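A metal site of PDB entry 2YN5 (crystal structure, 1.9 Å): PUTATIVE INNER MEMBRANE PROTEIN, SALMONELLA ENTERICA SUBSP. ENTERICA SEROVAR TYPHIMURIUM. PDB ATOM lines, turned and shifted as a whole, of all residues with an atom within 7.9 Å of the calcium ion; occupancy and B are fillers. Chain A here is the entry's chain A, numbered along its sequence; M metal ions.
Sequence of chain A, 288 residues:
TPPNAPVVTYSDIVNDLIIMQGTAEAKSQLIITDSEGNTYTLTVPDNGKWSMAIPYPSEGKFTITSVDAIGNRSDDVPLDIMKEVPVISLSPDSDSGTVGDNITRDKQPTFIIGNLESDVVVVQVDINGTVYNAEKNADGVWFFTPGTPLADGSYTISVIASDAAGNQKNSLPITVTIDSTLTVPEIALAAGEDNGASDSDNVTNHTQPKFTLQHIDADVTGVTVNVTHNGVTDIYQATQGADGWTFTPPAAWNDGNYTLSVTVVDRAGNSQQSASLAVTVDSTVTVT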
ATOM      1  N   LEU A 189      35.201   0.331  -9.276  1.00  0.00           N
ATOM      2  CA  LEU A 189      34.060   0.867  -8.538  1.00  0.00           C
ATOM      3  C   LEU A 189      34.259   0.473  -7.070  1.00  0.00           C
ATOM      4  O   LEU A 189      34.623  -0.664  -6.776  1.00  0.00           O
ATOM      5  CB  LEU A 189      32.743   0.331  -9.104  1.00  0.00           C
ATOM      6  CG  LEU A 189      32.175   0.979 -10.377  1.00  0.00           C
ATOM      7  CD1 LEU A 189      31.164   0.055 -11.005  1.00  0.00           C
ATOM      8  CD2 LEU A 189      31.544   2.334 -10.066  1.00  0.00           C
ATOM      9  N   GLU A 193      29.084   0.237  -4.862  1.00  0.00           N
ATOM     10  CA  GLU A 193      28.823   1.112  -6.034  1.00  0.00           C
ATOM     11  C   GLU A 193      28.461   0.295  -7.276  1.00  0.00           C
ATOM     12  O   GLU A 193      27.597   0.700  -8.056  1.00  0.00           O
ATOM     13  CB  GLU A 193      30.006   2.044  -6.298  1.00  0.00           C
ATOM     14  CG  GLU A 193      30.317   3.012  -5.161  1.00  0.00           C
ATOM     15  CD  GLU A 193      29.249   4.094  -4.954  1.00  0.00           C
ATOM     16  OE1 GLU A 193      29.059   4.935  -5.855  1.00  0.00           O
ATOM     17  OE2 GLU A 193      28.601   4.108  -3.880  1.00  0.00           O
ATOM     18  N   ASP A 194      29.116  -0.854  -7.457  1.00  0.00           N
ATOM     19  CA  ASP A 194      28.681  -1.810  -8.474  1.00  0.00           C
ATOM     20  C   ASP A 194      27.467  -2.548  -7.904  1.00  0.00           C
ATOM     21  O   ASP A 194      27.594  -3.637  -7.319  1.00  0.00           O
ATOM     22  CB  ASP A 194      29.809  -2.770  -8.901  1.00  0.00           C
ATOM     23  CG  ASP A 194      29.478  -3.519 -10.193  1.00  0.00           C
ATOM     24  OD1 ASP A 194      28.336  -3.340 -10.660  1.00  0.00           O
ATOM     25  OD2 ASP A 194      30.332  -4.262 -10.742  1.00  0.00           O
ATOM     26  N   ASN A 195      26.287  -1.935  -8.070  1.00  0.00           N
ATOM     27  CA  ASN A 195      25.054  -2.368  -7.394  1.00  0.00           C
ATOM     28  C   ASN A 195      23.976  -2.950  -8.339  1.00  0.00           C
ATOM     29  O   ASN A 195      24.300  -3.416  -9.432  1.00  0.00           O
ATOM     30  CB  ASN A 195      24.498  -1.233  -6.504  1.00  0.00           C
ATOM     31  CG  ASN A 195      24.073   0.010  -7.296  1.00  0.00           C
ATOM     32  OD1 ASN A 195      24.155   0.061  -8.526  1.00  0.00           O
ATOM     33  ND2 ASN A 195      23.615   1.024  -6.569  1.00  0.00           N
ATOM     34  N   GLY A 196      22.707  -2.912  -7.927  1.00  0.00           N
ATOM     35  CA  GLY A 196      21.624  -3.402  -8.773  1.00  0.00           C
ATOM     36  C   GLY A 196      21.589  -4.910  -8.785  1.00  0.00           C
ATOM     37  O   GLY A 196      21.579  -5.546  -7.733  1.00  0.00           O
ATOM     38  N   ALA A 197      21.579  -5.500  -9.988  1.00  0.00           N
ATOM     39  CA  ALA A 197      21.526  -6.951 -10.162  1.00  0.00           C
ATOM     40  C   ALA A 197      22.826  -7.665  -9.774  1.00  0.00           C
ATOM     41  O   ALA A 197      22.810  -8.574  -8.945  1.00  0.00           O
ATOM     42  CB  ALA A 197      21.118  -7.310 -11.587  1.00  0.00           C
ATOM     43  N   SER A 198      23.941  -7.249 -10.379  1.00  0.00           N
ATOM     44  CA  SER A 198      25.235  -7.914 -10.191  1.00  0.00           C
ATOM     45  C   SER A 198      26.290  -7.007  -9.562  1.00  0.00           C
ATOM     46  O   SER A 198      26.403  -5.824  -9.923  1.00  0.00           O
ATOM     47  CB  SER A 198      25.741  -8.485 -11.514  1.00  0.00           C
ATOM     48  OG  SER A 198      27.019  -9.106 -11.347  1.00  0.00           O
ATOM     49  N   ASP A 199      27.076  -7.562  -8.644  1.00  0.00           N
ATOM     50  CA  ASP A 199      28.147  -6.835  -7.976  1.00  0.00           C
ATOM     51  C   ASP A 199      29.444  -6.798  -8.807  1.00  0.00           C
ATOM     52  O   ASP A 199      30.458  -6.231  -8.360  1.00  0.00           O
ATOM     53  CB  ASP A 199      28.443  -7.482  -6.619  1.00  0.00           C
ATOM     54  CG  ASP A 199      29.211  -8.789  -6.755  1.00  0.00           C
ATOM     55  OD1 ASP A 199      28.723  -9.702  -7.462  1.00  0.00           O
ATOM     56  OD2 ASP A 199      30.310  -8.890  -6.185  1.00  0.00           O
ATOM     57  N   SER A 200      29.410  -7.423  -9.994  1.00  0.00           N
ATOM     58  CA  SER A 200      30.600  -7.664 -10.830  1.00  0.00           C
ATOM     59  C   SER A 200      30.496  -7.163 -12.284  1.00  0.00           C
ATOM     60  O   SER A 200      31.483  -7.239 -13.028  1.00  0.00           O
ATOM     61  CB  SER A 200      30.919  -9.155 -10.838  1.00  0.00           C
ATOM     62  OG  SER A 200      31.179  -9.630  -9.525  1.00  0.00           O
ATOM     63  N   ASP A 201      29.332  -6.680 -12.688  1.00  0.00           N
ATOM     64  CA  ASP A 201      29.108  -6.324 -14.084  1.00  0.00           C
ATOM     65  C   ASP A 201      29.505  -4.898 -14.475  1.00  0.00           C
ATOM     66  O   ASP A 201      29.462  -4.555 -15.654  1.00  0.00           O
ATOM     67  CB  ASP A 201      27.654  -6.644 -14.536  1.00  0.00           C
ATOM     68  CG  ASP A 201      26.579  -5.865 -13.758  1.00  0.00           C
ATOM     69  OD1 ASP A 201      26.861  -4.988 -12.902  1.00  0.00           O
ATOM     70  OD2 ASP A 201      25.390  -6.172 -14.015  1.00  0.00           O
ATOM     71  N   ASN A 202      29.887  -4.084 -13.493  1.00  0.00           N
ATOM     72  CA  ASN A 202      30.236  -2.674 -13.723  1.00  0.00           C
ATOM     73  C   ASN A 202      29.078  -1.830 -14.289  1.00  0.00           C
ATOM     74  O   ASN A 202      29.281  -0.827 -14.969  1.00  0.00           O
ATOM     75  CB  ASN A 202      31.500  -2.559 -14.609  1.00  0.00           C
ATOM     76  CG  ASN A 202      32.745  -3.061 -13.892  1.00  0.00           C
ATOM     77  OD1 ASN A 202      32.973  -2.731 -12.732  1.00  0.00           O
ATOM     78  ND2 ASN A 202      33.565  -3.831 -14.594  1.00  0.00           N
ATOM     79  N   VAL A 203      27.845  -2.273 -13.996  1.00  0.00           N
ATOM     80  CA  VAL A 203      26.654  -1.470 -14.236  1.00  0.00           C
ATOM     81  C   VAL A 203      26.197  -0.948 -12.873  1.00  0.00           C
ATOM     82  O   VAL A 203      25.961  -1.738 -11.961  1.00  0.00           O
ATOM     83  CB  VAL A 203      25.531  -2.283 -14.902  1.00  0.00           C
ATOM     84  CG1 VAL A 203      24.274  -1.436 -15.109  1.00  0.00           C
ATOM     85  CG2 VAL A 203      26.009  -2.842 -16.223  1.00  0.00           C
ATOM     86  N   THR A 204      26.115   0.371 -12.755  1.00  0.00           N
ATOM     87  CA  THR A 204      25.698   1.014 -11.506  1.00  0.00           C
ATOM     88  C   THR A 204      24.424   1.798 -11.745  1.00  0.00           C
ATOM     89  O   THR A 204      24.137   2.227 -12.877  1.00  0.00           O
ATOM     90  CB  THR A 204      26.792   1.939 -10.936  1.00  0.00           C
ATOM     91  OG1 THR A 204      26.364   2.503  -9.691  1.00  0.00           O
ATOM     92  CG2 THR A 204      27.151   3.088 -11.918  1.00  0.00           C
ATOM     93  N   ASN A 205      23.621   1.950 -10.700  1.00  0.00           N
ATOM     94  CA  ASN A 205      22.479   2.859 -10.774  1.00  0.00           C
ATOM     95  C   ASN A 205      22.762   4.211 -10.109  1.00  0.00           C
ATOM     96  O   ASN A 205      21.889   5.074 -10.051  1.00  0.00           O
ATOM     97  CB  ASN A 205      21.168   2.216 -10.284  1.00  0.00           C
ATOM     98  CG  ASN A 205      21.256   1.673  -8.861  1.00  0.00           C
ATOM     99  OD1 ASN A 205      21.792   2.334  -7.961  1.00  0.00           O
ATOM    100  ND2 ASN A 205      20.706   0.480  -8.653  1.00  0.00           N
ATOM    101  N   THR A 280      28.778   1.104 -17.009  1.00  0.00           N
ATOM    102  CA  THR A 280      27.482   1.573 -17.501  1.00  0.00           C
ATOM    103  C   THR A 280      26.703   2.183 -16.331  1.00  0.00           C
ATOM    104  O   THR A 280      26.597   1.581 -15.246  1.00  0.00           O
ATOM    105  CB  THR A 280      26.670   0.444 -18.158  1.00  0.00           C
ATOM    106  OG1 THR A 280      27.483  -0.176 -19.158  1.00  0.00           O
ATOM    107  CG2 THR A 280      25.391   0.980 -18.802  1.00  0.00           C
HETATM  108 CA    CA M   1      25.994  -3.838 -10.939  1.00  0.00          CA
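OG of Ser 198 lies close to N of Ser 200. The side-chain amide oxygen (OD1) of Asn 195 lies close to the side-chain hydroxyl (OG1) of Thr 204. The side-chain amide nitrogen of Asn 195 sits at hydrogen-bond distance from the side-chain amide oxygen of Asn 205 (2.6 Å). N of Asn 202 sits at hydrogen-bond distance from OD2 of Asp 194, 2.8 Å away. The backbone NH of Ser 200 sits close to the side-chain carboxylate of Asp 194.
The calcium ion is bound by the backbone carbonyl oxygen (O) of Ser 198 (2.3 Å), the backbone carbonyl oxygen (O) of Asn 195 (2.3 Å), the backbone carbonyl oxygen (O) of Val 203 (2.3 Å), the side-chain carboxylate (OD1) of Asp 194 (2.4 Å) and the side-chain carboxylate (OD1) of Asp 201 (2.4 Å).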
